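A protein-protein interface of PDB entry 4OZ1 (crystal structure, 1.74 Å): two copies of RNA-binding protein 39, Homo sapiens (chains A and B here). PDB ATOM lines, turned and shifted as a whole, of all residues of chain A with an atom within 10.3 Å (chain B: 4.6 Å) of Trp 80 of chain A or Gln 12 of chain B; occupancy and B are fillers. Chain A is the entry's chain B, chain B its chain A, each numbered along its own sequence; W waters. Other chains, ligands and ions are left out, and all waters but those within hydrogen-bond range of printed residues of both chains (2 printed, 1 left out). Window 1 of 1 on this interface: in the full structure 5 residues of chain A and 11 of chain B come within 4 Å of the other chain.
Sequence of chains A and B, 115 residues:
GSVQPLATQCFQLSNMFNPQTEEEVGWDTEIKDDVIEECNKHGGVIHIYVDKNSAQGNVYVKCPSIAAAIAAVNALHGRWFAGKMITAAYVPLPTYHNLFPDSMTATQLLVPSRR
Of chain B, only Gln 12, Ala 89 and Tyr 90 come within 4 Å of Trp 80 of chain A. Gln 12 of chain B touches three residues of chain A. No residue of chain A comes within 4 Å of Leu 13 of chain B. No residue of chain A comes within 4 Å of Ala 88 of chain B. Ala 89 of chain B touches one residue of chain A. Of the printed residues of chain B, His 77 of chain A touches Asn 58 (3.9 Å). Of the printed residues of chain A, Asn 58 of chain B touches His 77 (3.9 Å). Of the printed residues of chain A, Tyr 60 of chain B touches Gly 78 and Met 85. The nearest printed residue of chain B that does not touch His 77 of chain A is Tyr 60 of chain B (4.5 Å).
4 positions are printed for both chains.
Hydrophobic or aromatic side chains of chain B within 4 Å of the printed part of chain A: Tyr 60 and Ala 89. Among the printed residues, 8 pairs touch across the chains. Among the printed residues, no Asp or Glu carboxylate lies within 4 Å of a Lys or Arg side-chain nitrogen of the other chain.
Among the printed residues, merely in contact across the chains: His 77 of chain A with Asn 58 of chain B (3.9 Å), Gly 78 of chain A with Tyr 60 of chain B (3.3 Å), Trp 80 of chain A with Ala 89 of chain B (3.9 Å), Trp 80 of chain A with Tyr 90 of chain B (3.3 Å) and Met 85 of chain A with Tyr 60 of chain B (3.9 Å).
Water W2 lies within hydrogen-bond range of the backbone carbonyl oxygen (O) of His 77 of chain A, the side-chain amide nitrogen (ND2) of Asn 58 of chain B and the backbone NH (N) of Arg 79 of chain A. Water W1 lies within hydrogen-bond range of OH of Tyr 60 of chain B (2.8 Å), ND2 of Asn 58 of chain B (3.0 Å) and ND1 of His 77 of chain A (3.4 Å).
The side-chain amide nitrogen (NE2) of Gln 12 of chain B sits at hydrogen-bond distance from the side-chain hydroxyl (OH) of Tyr 60 of chain B. O of Ala 89 of chain B sits at hydrogen-bond distance from N of Gln 12 of chain B, at 2.7 Å. O of Leu 13 of chain B lies close to OD1 of Asn 58 of chain B, at 3.5 Å. OG of Ser 14 of chain B is in hydrogen-bond range of OD1 of Asn 58 of chain B, 3.0 Å away. The side-chain amide nitrogen (ND2) of Asn 15 of chain A lies within hydrogen-bond range of the backbone carbonyl oxygen (O) of Met 85 of chain A (2.9 Å). The backbone NH of Gly 78 of chain A is in hydrogen-bond range of the backbone carbonyl oxygen of Ile 86 of chain A, at 2.9 Å.
The side-chain amide nitrogen (NE2) of Gln 12 of chain B is in hydrogen-bond range of the backbone carbonyl oxygen (O) of Gly 78 of chain A, 2.8 Å away. The side-chain amide oxygen of Gln 12 of chain B lies within hydrogen-bond range of the indole nitrogen of Trp 80 of chain A, 3.4 Å away. The side-chain sulfur (SD) of Met 85 of chain A sits at hydrogen-bond distance from the side-chain amide nitrogen (NE2) of Gln 12 of chain B (3.8 Å).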
ATOM      1  N   LEU A  13     -10.550   1.010  16.304  1.00  0.00           N
ATOM      2  CA  LEU A  13      -9.692   1.437  17.402  1.00  0.00           C
ATOM      3  C   LEU A  13     -10.581   1.849  18.569  1.00  0.00           C
ATOM      4  O   LEU A  13     -11.621   2.462  18.342  1.00  0.00           O
ATOM      5  CB  LEU A  13      -8.808   2.616  16.975  1.00  0.00           C
ATOM      6  CG  LEU A  13      -7.867   2.374  15.803  1.00  0.00           C
ATOM      7  CD1 LEU A  13      -7.194   3.667  15.352  1.00  0.00           C
ATOM      8  CD2 LEU A  13      -6.850   1.348  16.189  1.00  0.00           C
ATOM      9  N   SER A  14     -10.193   1.479  19.790  1.00  0.00           N
ATOM     10  CA  SER A  14     -10.889   1.921  20.999  1.00  0.00           C
ATOM     11  C   SER A  14      -9.942   2.625  21.969  1.00  0.00           C
ATOM     12  O   SER A  14      -8.708   2.543  21.855  1.00  0.00           O
ATOM     13  CB  SER A  14     -11.574   0.746  21.692  1.00  0.00           C
ATOM     14  OG  SER A  14     -12.551   1.196  22.628  1.00  0.00           O
ATOM     15  N   ASN A  15     -10.548   3.349  22.905  1.00  0.00           N
ATOM     16  CA  ASN A  15      -9.829   4.058  23.975  1.00  0.00           C
ATOM     17  C   ASN A  15      -9.023   5.236  23.413  1.00  0.00           C
ATOM     18  O   ASN A  15      -8.073   5.704  24.041  1.00  0.00           O
ATOM     19  CB  ASN A  15      -8.927   3.095  24.740  1.00  0.00           C
ATOM     20  CG  ASN A  15      -8.828   3.422  26.211  1.00  0.00           C
ATOM     21  OD1 ASN A  15      -9.692   4.109  26.768  1.00  0.00           O
ATOM     22  ND2 ASN A  15      -7.773   2.937  26.853  1.00  0.00           N
ATOM     23  N   MET A  16      -9.426   5.732  22.246  1.00  0.00           N
ATOM     24  CA  MET A  16      -8.719   6.821  21.562  1.00  0.00           C
ATOM     25  C   MET A  16      -9.028   8.220  22.091  1.00  0.00           C
ATOM     26  O   MET A  16      -8.318   9.162  21.760  1.00  0.00           O
ATOM     27  CB  MET A  16      -9.041   6.805  20.055  1.00  0.00           C
ATOM     28  CG  MET A  16      -8.440   5.628  19.286  1.00  0.00           C
ATOM     29  SD  MET A  16      -6.659   5.701  19.108  1.00  0.00           S
ATOM     30  CE  MET A  16      -6.481   7.039  17.929  1.00  0.00           C
ATOM     31  N   PHE A  17     -10.096   8.355  22.875  1.00  0.00           N
ATOM     32  CA  PHE A  17     -10.526   9.624  23.428  1.00  0.00           C
ATOM     33  C   PHE A  17     -11.608   9.316  24.441  1.00  0.00           C
ATOM     34  O   PHE A  17     -12.010   8.165  24.595  1.00  0.00           O
ATOM     35  CB  PHE A  17     -11.047  10.597  22.346  1.00  0.00           C
ATOM     36  CG  PHE A  17     -12.175  10.056  21.489  1.00  0.00           C
ATOM     37  CD1 PHE A  17     -11.906   9.331  20.339  1.00  0.00           C
ATOM     38  CD2 PHE A  17     -13.499  10.324  21.805  1.00  0.00           C
ATOM     39  CE1 PHE A  17     -12.939   8.834  19.549  1.00  0.00           C
ATOM     40  CE2 PHE A  17     -14.534   9.845  21.016  1.00  0.00           C
ATOM     41  CZ  PHE A  17     -14.246   9.099  19.875  1.00  0.00           C
ATOM     42  N   ASP A  34      -4.058  11.974  13.090  1.00  0.00           N
ATOM     43  CA  ASP A  34      -3.049  11.123  13.709  1.00  0.00           C
ATOM     44  C   ASP A  34      -3.173   9.695  13.201  1.00  0.00           C
ATOM     45  O   ASP A  34      -2.170   8.992  13.031  1.00  0.00           O
ATOM     46  CB  ASP A  34      -3.158  11.142  15.237  1.00  0.00           C
ATOM     47  CG  ASP A  34      -2.572  12.411  15.870  1.00  0.00           C
ATOM     48  OD1 ASP A  34      -2.046  13.281  15.142  1.00  0.00           O
ATOM     49  OD2 ASP A  34      -2.610  12.508  17.125  1.00  0.00           O
ATOM     50  N   GLU A  37      -1.901   9.717   9.514  1.00  0.00           N
ATOM     51  CA  GLU A  37      -0.445   9.803   9.500  1.00  0.00           C
ATOM     52  C   GLU A  37       0.185   8.447   9.826  1.00  0.00           C
ATOM     53  O   GLU A  37       1.140   8.010   9.174  1.00  0.00           O
ATOM     54  CB  GLU A  37       0.003  10.876  10.505  1.00  0.00           C
ATOM     55  CG  GLU A  37       1.500  10.944  10.777  1.00  0.00           C
ATOM     56  CD  GLU A  37       1.811  11.012  12.261  1.00  0.00           C
ATOM     57  OE1 GLU A  37       2.128  12.122  12.746  1.00  0.00           O
ATOM     58  OE2 GLU A  37       1.733   9.957  12.936  1.00  0.00           O
ATOM     59  N   GLU A  38      -0.355   7.731  10.804  1.00  0.00           N
ATOM     60  CA  GLU A  38       0.225   6.430  11.099  1.00  0.00           C
ATOM     61  C   GLU A  38      -0.064   5.413  10.000  1.00  0.00           C
ATOM     62  O   GLU A  38       0.802   4.592   9.679  1.00  0.00           O
ATOM     63  CB  GLU A  38      -0.247   5.886  12.449  1.00  0.00           C
ATOM     64  CG  GLU A  38       0.473   6.484  13.623  1.00  0.00           C
ATOM     65  CD  GLU A  38       1.973   6.205  13.607  1.00  0.00           C
ATOM     66  OE1 GLU A  38       2.373   5.031  13.467  1.00  0.00           O
ATOM     67  OE2 GLU A  38       2.754   7.170  13.730  1.00  0.00           O
ATOM     68  N   VAL A  73      -2.985  -2.487  12.005  1.00  0.00           N
ATOM     69  CA  VAL A  73      -3.441  -3.075  13.259  1.00  0.00           C
ATOM     70  C   VAL A  73      -2.279  -3.555  14.104  1.00  0.00           C
ATOM     71  O   VAL A  73      -2.246  -3.317  15.322  1.00  0.00           O
ATOM     72  CB  VAL A  73      -4.424  -4.234  13.001  1.00  0.00           C
ATOM     73  CG1 VAL A  73      -4.611  -5.107  14.227  1.00  0.00           C
ATOM     74  CG2 VAL A  73      -5.798  -3.685  12.555  1.00  0.00           C
ATOM     75  N   ASN A  74      -1.324  -4.238  13.471  1.00  0.00           N
ATOM     76  CA  ASN A  74      -0.193  -4.787  14.221  1.00  0.00           C
ATOM     77  C   ASN A  74       0.730  -3.693  14.730  1.00  0.00           C
ATOM     78  O   ASN A  74       1.521  -3.917  15.663  1.00  0.00           O
ATOM     79  CB  ASN A  74       0.596  -5.774  13.363  1.00  0.00           C
ATOM     80  CG  ASN A  74      -0.203  -7.039  13.050  1.00  0.00           C
ATOM     81  OD1 ASN A  74      -1.152  -7.393  13.764  1.00  0.00           O
ATOM     82  ND2 ASN A  74       0.149  -7.696  11.959  1.00  0.00           N
ATOM     83  N   ALA A  75       0.696  -2.538  14.065  1.00  0.00           N
ATOM     84  CA  ALA A  75       1.432  -1.358  14.537  1.00  0.00           C
ATOM     85  C   ALA A  75       0.691  -0.563  15.621  1.00  0.00           C
ATOM     86  O   ALA A  75       1.321   0.130  16.420  1.00  0.00           O
ATOM     87  CB  ALA A  75       1.777  -0.439  13.357  1.00  0.00           C
ATOM     88  N   LEU A  76      -0.634  -0.613  15.618  1.00  0.00           N
ATOM     89  CA  LEU A  76      -1.446   0.223  16.512  1.00  0.00           C
ATOM     90  C   LEU A  76      -2.015  -0.456  17.770  1.00  0.00           C
ATOM     91  O   LEU A  76      -2.245   0.234  18.793  1.00  0.00           O
ATOM     92  CB  LEU A  76      -2.594   0.860  15.731  1.00  0.00           C
ATOM     93  CG  LEU A  76      -2.179   1.812  14.602  1.00  0.00           C
ATOM     94  CD1 LEU A  76      -3.402   2.259  13.855  1.00  0.00           C
ATOM     95  CD2 LEU A  76      -1.332   2.986  15.032  1.00  0.00           C
ATOM     96  N   HIS A  77      -2.326  -1.756  17.687  1.00  0.00           N
ATOM     97  CA  HIS A  77      -2.884  -2.456  18.835  1.00  0.00           C
ATOM     98  C   HIS A  77      -1.840  -2.440  19.946  1.00  0.00           C
ATOM     99  O   HIS A  77      -0.694  -2.800  19.711  1.00  0.00           O
ATOM    100  CB  HIS A  77      -3.256  -3.907  18.462  1.00  0.00           C
ATOM    101  CG  HIS A  77      -3.928  -4.659  19.573  1.00  0.00           C
ATOM    102  ND1 HIS A  77      -3.405  -5.814  20.111  1.00  0.00           N
ATOM    103  CD2 HIS A  77      -5.066  -4.415  20.259  1.00  0.00           C
ATOM    104  CE1 HIS A  77      -4.196  -6.255  21.071  1.00  0.00           C
ATOM    105  NE2 HIS A  77      -5.206  -5.416  21.191  1.00  0.00           N
ATOM    106  N   GLY A  78      -2.226  -2.064  21.162  1.00  0.00           N
ATOM    107  CA  GLY A  78      -1.278  -2.076  22.274  1.00  0.00           C
ATOM    108  C   GLY A  78      -0.461  -0.797  22.362  1.00  0.00           C
ATOM    109  O   GLY A  78       0.331  -0.562  23.293  1.00  0.00           O
ATOM    110  N   ARG A  79      -0.642   0.061  21.368  1.00  0.00           N
ATOM    111  CA  ARG A  79       0.027   1.344  21.371  1.00  0.00           C
ATOM    112  C   ARG A  79      -0.622   2.342  22.338  1.00  0.00           C
ATOM    113  O   ARG A  79      -1.821   2.336  22.558  1.00  0.00           O
ATOM    114  CB  ARG A  79       0.003   1.890  19.955  1.00  0.00           C
ATOM    115  CG  ARG A  79       0.953   2.988  19.657  1.00  0.00           C
ATOM    116  CD  ARG A  79       2.157   2.497  18.884  1.00  0.00           C
ATOM    117  NE  ARG A  79       2.878   3.658  18.370  1.00  0.00           N
ATOM    118  CZ  ARG A  79       2.987   3.969  17.081  1.00  0.00           C
ATOM    119  NH1 ARG A  79       2.472   3.182  16.137  1.00  0.00           N
ATOM    120  NH2 ARG A  79       3.645   5.058  16.736  1.00  0.00           N
ATOM    121  N   TRP A  80       0.166   3.277  22.829  1.00  0.00           N
ATOM    122  CA  TRP A  80      -0.353   4.277  23.723  1.00  0.00           C
ATOM    123  C   TRP A  80      -0.711   5.496  22.885  1.00  0.00           C
ATOM    124  O   TRP A  80      -0.018   5.822  21.967  1.00  0.00           O
ATOM    125  CB  TRP A  80       0.671   4.575  24.807  1.00  0.00           C
ATOM    126  CG  TRP A  80       0.797   3.391  25.695  1.00  0.00           C
ATOM    127  CD1 TRP A  80       1.469   2.224  25.441  1.00  0.00           C
ATOM    128  CD2 TRP A  80       0.185   3.238  26.965  1.00  0.00           C
ATOM    129  NE1 TRP A  80       1.317   1.351  26.500  1.00  0.00           N
ATOM    130  CE2 TRP A  80       0.539   1.957  27.454  1.00  0.00           C
ATOM    131  CE3 TRP A  80      -0.615   4.064  27.750  1.00  0.00           C
ATOM    132  CZ2 TRP A  80       0.108   1.487  28.687  1.00  0.00           C
ATOM    133  CZ3 TRP A  80      -1.036   3.604  28.970  1.00  0.00           C
ATOM    134  CH2 TRP A  80      -0.671   2.323  29.434  1.00  0.00           C
ATOM    135  N   PHE A  81      -1.878   6.056  23.118  1.00  0.00           N
ATOM    136  CA  PHE A  81      -2.330   7.259  22.412  1.00  0.00           C
ATOM    137  C   PHE A  81      -2.947   8.213  23.417  1.00  0.00           C
ATOM    138  O   PHE A  81      -3.867   7.827  24.133  1.00  0.00           O
ATOM    139  CB  PHE A  81      -3.345   6.924  21.327  1.00  0.00           C
ATOM    140  CG  PHE A  81      -3.799   8.119  20.548  1.00  0.00           C
ATOM    141  CD1 PHE A  81      -3.024   8.622  19.521  1.00  0.00           C
ATOM    142  CD2 PHE A  81      -4.987   8.756  20.853  1.00  0.00           C
ATOM    143  CE1 PHE A  81      -3.419   9.737  18.810  1.00  0.00           C
ATOM    144  CE2 PHE A  81      -5.393   9.870  20.150  1.00  0.00           C
ATOM    145  CZ  PHE A  81      -4.602  10.367  19.124  1.00  0.00           C
ATOM    146  N   ALA A  82      -2.451   9.439  23.484  1.00  0.00           N
ATOM    147  CA  ALA A  82      -3.021  10.462  24.381  1.00  0.00           C
ATOM    148  C   ALA A  82      -3.121   9.976  25.819  1.00  0.00           C
ATOM    149  O   ALA A  82      -4.052  10.350  26.553  1.00  0.00           O
ATOM    150  CB  ALA A  82      -4.403  10.900  23.875  1.00  0.00           C
ATOM    151  N   GLY A  83      -2.119   9.209  26.233  1.00  0.00           N
ATOM    152  CA  GLY A  83      -2.012   8.728  27.598  1.00  0.00           C
ATOM    153  C   GLY A  83      -2.796   7.461  27.919  1.00  0.00           C
ATOM    154  O   GLY A  83      -2.914   7.116  29.079  1.00  0.00           O
ATOM    155  N   LYS A  84      -3.385   6.818  26.911  1.00  0.00           N
ATOM    156  CA  LYS A  84      -4.154   5.591  27.119  1.00  0.00           C
ATOM    157  C   LYS A  84      -3.736   4.461  26.186  1.00  0.00           C
ATOM    158  O   LYS A  84      -3.356   4.716  25.040  1.00  0.00           O
ATOM    159  CB  LYS A  84      -5.642   5.885  26.947  1.00  0.00           C
ATOM    160  CG  LYS A  84      -6.203   6.768  28.074  1.00  0.00           C
ATOM    161  CD  LYS A  84      -7.703   6.943  27.979  1.00  0.00           C
ATOM    162  CE  LYS A  84      -8.239   7.799  29.131  1.00  0.00           C
ATOM    163  NZ  LYS A  84      -9.729   7.798  29.164  1.00  0.00           N
ATOM    164  N   MET A  85      -3.858   3.208  26.642  1.00  0.00           N
ATOM    165  CA  MET A  85      -3.522   2.076  25.776  1.00  0.00           C
ATOM    166  C   MET A  85      -4.706   1.747  24.881  1.00  0.00           C
ATOM    167  O   MET A  85      -5.816   1.454  25.328  1.00  0.00           O
ATOM    168  CB  MET A  85      -3.118   0.854  26.579  1.00  0.00           C
ATOM    169  CG  MET A  85      -2.422  -0.163  25.705  1.00  0.00           C
ATOM    170  SD  MET A  85      -2.092  -1.684  26.573  1.00  0.00           S
ATOM    171  CE  MET A  85      -3.683  -2.470  26.402  1.00  0.00           C
ATOM    172  N   ILE A  86      -4.418   1.827  23.601  1.00  0.00           N
ATOM    173  CA  ILE A  86      -5.330   1.554  22.502  1.00  0.00           C
ATOM    174  C   ILE A  86      -5.504   0.092  22.154  1.00  0.00           C
ATOM    175  O   ILE A  86      -4.537  -0.682  22.200  1.00  0.00           O
ATOM    176  CB  ILE A  86      -4.845   2.314  21.232  1.00  0.00           C
ATOM    177  CG1 ILE A  86      -4.767   3.819  21.504  1.00  0.00           C
ATOM    178  CG2 ILE A  86      -5.696   2.021  20.010  1.00  0.00           C
ATOM    179  CD1 ILE A  86      -5.896   4.396  22.347  1.00  0.00           C
ATOM    180  N   THR A  87      -6.732  -0.298  21.819  1.00  0.00           N
ATOM    181  CA  THR A  87      -6.901  -1.636  21.254  1.00  0.00           C
ATOM    182  C   THR A  87      -7.502  -1.519  19.859  1.00  0.00           C
ATOM    183  O   THR A  87      -8.178  -0.525  19.544  1.00  0.00           O
ATOM    184  CB  THR A  87      -7.741  -2.535  22.158  1.00  0.00           C
ATOM    185  OG1 THR A  87      -8.948  -1.873  22.473  1.00  0.00           O
ATOM    186  CG2 THR A  87      -7.028  -2.797  23.436  1.00  0.00           C
ATOM    187  N   ALA A  88      -7.164  -2.485  19.005  1.00  0.00           N
ATOM    188  CA  ALA A  88      -7.621  -2.552  17.625  1.00  0.00           C
ATOM    189  C   ALA A  88      -8.254  -3.916  17.461  1.00  0.00           C
ATOM    190  O   ALA A  88      -7.712  -4.943  17.940  1.00  0.00           O
ATOM    191  CB  ALA A  88      -6.487  -2.360  16.642  1.00  0.00           C
ATOM    192  N   PHE B  11       1.144  -5.201  33.366  1.00  0.00           N
ATOM    193  CA  PHE B  11       2.037  -4.418  32.505  1.00  0.00           C
ATOM    194  C   PHE B  11       2.210  -4.999  31.123  1.00  0.00           C
ATOM    195  O   PHE B  11       1.847  -6.129  30.842  1.00  0.00           O
ATOM    196  CB  PHE B  11       3.412  -4.242  33.165  1.00  0.00           C
ATOM    197  CG  PHE B  11       4.135  -5.529  33.495  1.00  0.00           C
ATOM    198  CD1 PHE B  11       3.912  -6.189  34.690  1.00  0.00           C
ATOM    199  CD2 PHE B  11       5.096  -6.040  32.633  1.00  0.00           C
ATOM    200  CE1 PHE B  11       4.606  -7.369  35.002  1.00  0.00           C
ATOM    201  CE2 PHE B  11       5.794  -7.215  32.940  1.00  0.00           C
ATOM    202  CZ  PHE B  11       5.541  -7.880  34.115  1.00  0.00           C
ATOM    203  N   GLN B  12       2.752  -4.160  30.253  1.00  0.00           N
ATOM    204  CA  GLN B  12       3.043  -4.508  28.865  1.00  0.00           C
ATOM    205  C   GLN B  12       4.528  -4.330  28.648  1.00  0.00           C
ATOM    206  O   GLN B  12       5.051  -3.234  28.874  1.00  0.00           O
ATOM    207  CB  GLN B  12       2.273  -3.614  27.920  1.00  0.00           C
ATOM    208  CG  GLN B  12       2.550  -3.836  26.448  1.00  0.00           C
ATOM    209  CD  GLN B  12       2.207  -2.609  25.644  1.00  0.00           C
ATOM    210  OE1 GLN B  12       2.894  -1.596  25.718  1.00  0.00           O
ATOM    211  NE2 GLN B  12       1.123  -2.676  24.888  1.00  0.00           N
ATOM    212  N   LEU B  13       5.198  -5.403  28.250  1.00  0.00           N
ATOM    213  CA  LEU B  13       6.585  -5.331  27.806  1.00  0.00           C
ATOM    214  C   LEU B  13       6.605  -5.073  26.314  1.00  0.00           C
ATOM    215  O   LEU B  13       5.768  -5.613  25.597  1.00  0.00           O
ATOM    216  CB  LEU B  13       7.330  -6.629  28.108  1.00  0.00           C
ATOM    217  CG  LEU B  13       7.427  -7.093  29.547  1.00  0.00           C
ATOM    218  CD1 LEU B  13       7.983  -8.479  29.555  1.00  0.00           C
ATOM    219  CD2 LEU B  13       8.300  -6.174  30.365  1.00  0.00           C
ATOM    220  N   SER B  14       7.550  -4.252  25.852  1.00  0.00           N
ATOM    221  CA  SER B  14       7.750  -4.024  24.425  1.00  0.00           C
ATOM    222  C   SER B  14       9.165  -4.441  24.041  1.00  0.00           C
ATOM    223  O   SER B  14      10.038  -4.516  24.911  1.00  0.00           O
ATOM    224  CB  SER B  14       7.536  -2.549  24.062  1.00  0.00           C
ATOM    225  OG  SER B  14       6.177  -2.174  24.188  1.00  0.00           O
ATOM    226  N   ASN B  58       5.014  -6.963  21.864  1.00  0.00           N
ATOM    227  CA  ASN B  58       4.331  -6.808  23.129  1.00  0.00           C
ATOM    228  C   ASN B  58       4.055  -8.135  23.809  1.00  0.00           C
ATOM    229  O   ASN B  58       3.580  -9.083  23.181  1.00  0.00           O
ATOM    230  CB  ASN B  58       3.015  -6.072  22.952  1.00  0.00           C
ATOM    231  CG  ASN B  58       3.189  -4.648  22.549  1.00  0.00           C
ATOM    232  OD1 ASN B  58       4.069  -3.948  23.041  1.00  0.00           O
ATOM    233  ND2 ASN B  58       2.331  -4.187  21.656  1.00  0.00           N
ATOM    234  N   VAL B  59       4.352  -8.176  25.100  1.00  0.00           N
ATOM    235  CA  VAL B  59       3.985  -9.282  25.967  1.00  0.00           C
ATOM    236  C   VAL B  59       3.189  -8.667  27.106  1.00  0.00           C
ATOM    237  O   VAL B  59       3.624  -7.675  27.673  1.00  0.00           O
ATOM    238  CB  VAL B  59       5.177 -10.030  26.531  1.00  0.00           C
ATOM    239  CG1 VAL B  59       4.726 -11.159  27.492  1.00  0.00           C
ATOM    240  CG2 VAL B  59       6.075 -10.601  25.425  1.00  0.00           C
ATOM    241  N   TYR B  60       2.013  -9.224  27.393  1.00  0.00           N
ATOM    242  CA  TYR B  60       1.148  -8.761  28.469  1.00  0.00           C
ATOM    243  C   TYR B  60       1.242  -9.691  29.665  1.00  0.00           C
ATOM    244  O   TYR B  60       1.188 -10.925  29.511  1.00  0.00           O
ATOM    245  CB  TYR B  60      -0.306  -8.658  27.985  1.00  0.00           C
ATOM    246  CG  TYR B  60      -0.456  -7.650  26.872  1.00  0.00           C
ATOM    247  CD1 TYR B  60      -0.211  -8.025  25.561  1.00  0.00           C
ATOM    248  CD2 TYR B  60      -0.815  -6.327  27.125  1.00  0.00           C
ATOM    249  CE1 TYR B  60      -0.334  -7.118  24.524  1.00  0.00           C
ATOM    250  CE2 TYR B  60      -0.930  -5.415  26.090  1.00  0.00           C
ATOM    251  CZ  TYR B  60      -0.671  -5.823  24.794  1.00  0.00           C
ATOM    252  OH  TYR B  60      -0.796  -4.949  23.742  1.00  0.00           O
ATOM    253  N   THR B  87      11.138  -2.626  27.313  1.00  0.00           N
ATOM    254  CA  THR B  87      10.518  -1.545  28.064  1.00  0.00           C
ATOM    255  C   THR B  87       9.220  -2.048  28.636  1.00  0.00           C
ATOM    256  O   THR B  87       8.579  -2.921  28.043  1.00  0.00           O
ATOM    257  CB  THR B  87      10.245  -0.298  27.175  1.00  0.00           C
ATOM    258  OG1 THR B  87       9.386  -0.658  26.101  1.00  0.00           O
ATOM    259  CG2 THR B  87      11.511   0.254  26.586  1.00  0.00           C
ATOM    260  N   ALA B  88       8.835  -1.503  29.785  1.00  0.00           N
ATOM    261  CA  ALA B  88       7.613  -1.915  30.455  1.00  0.00           C
ATOM    262  C   ALA B  88       6.721  -0.714  30.674  1.00  0.00           C
ATOM    263  O   ALA B  88       7.194   0.362  31.071  1.00  0.00           O
ATOM    264  CB  ALA B  88       7.926  -2.581  31.775  1.00  0.00           C
ATOM    265  N   ALA B  89       5.428  -0.897  30.429  1.00  0.00           N
ATOM    266  CA  ALA B  89       4.463   0.140  30.748  1.00  0.00           C
ATOM    267  C   ALA B  89       3.364  -0.526  31.552  1.00  0.00           C
ATOM    268  O   ALA B  89       2.851  -1.566  31.160  1.00  0.00           O
ATOM    269  CB  ALA B  89       3.897   0.801  29.463  1.00  0.00           C
ATOM    270  N   TYR B  90       3.009   0.073  32.685  1.00  0.00           N
ATOM    271  CA  TYR B  90       1.908  -0.445  33.483  1.00  0.00           C
ATOM    272  C   TYR B  90       0.608  -0.177  32.773  1.00  0.00           C
ATOM    273  O   TYR B  90       0.473   0.871  32.133  1.00  0.00           O
ATOM    274  CB  TYR B  90       1.908   0.179  34.887  1.00  0.00           C
ATOM    275  CG  TYR B  90       3.091  -0.292  35.699  1.00  0.00           C
ATOM    276  CD1 TYR B  90       3.128  -1.581  36.200  1.00  0.00           C
ATOM    277  CD2 TYR B  90       4.175   0.539  35.935  1.00  0.00           C
ATOM    278  CE1 TYR B  90       4.190  -2.036  36.925  1.00  0.00           C
ATOM    279  CE2 TYR B  90       5.265   0.085  36.671  1.00  0.00           C
ATOM    280  CZ  TYR B  90       5.253  -1.215  37.156  1.00  0.00           C
ATOM    281  OH  TYR B  90       6.303  -1.713  37.890  1.00  0.00           O
ATOM    282  N   VAL B  91      -0.324  -1.124  32.896  1.00  0.00           N
ATOM    283  CA  VAL B  91      -1.641  -1.034  32.280  1.00  0.00           C
ATOM    284  C   VAL B  91      -2.675  -0.907  33.393  1.00  0.00           C
ATOM    285  O   VAL B  91      -2.634  -1.656  34.361  1.00  0.00           O
ATOM    286  CB  VAL B  91      -1.937  -2.285  31.415  1.00  0.00           C
ATOM    287  CG1 VAL B  91      -3.277  -2.181  30.782  1.00  0.00           C
ATOM    288  CG2 VAL B  91      -0.857  -2.460  30.337  1.00  0.00           C
ATOM    289  N   PRO B  92      -3.579   0.082  33.299  1.00  0.00           N
ATOM    290  CA  PRO B  92      -4.642   0.132  34.305  1.00  0.00           C
ATOM    291  C   PRO B  92      -5.450  -1.159  34.324  1.00  0.00           C
ATOM    292  O   PRO B  92      -5.722  -1.740  33.271  1.00  0.00           O
ATOM    293  CB  PRO B  92      -5.495   1.310  33.854  1.00  0.00           C
ATOM    294  CG  PRO B  92      -4.540   2.179  33.100  1.00  0.00           C
ATOM    295  CD  PRO B  92      -3.609   1.252  32.406  1.00  0.00           C
HETATM  296  O   HOH W   1      -0.147  -5.898  21.199  1.00  0.00           O
HETATM  297  O   HOH W   2       1.759  -1.979  20.206  1.00  0.00           O
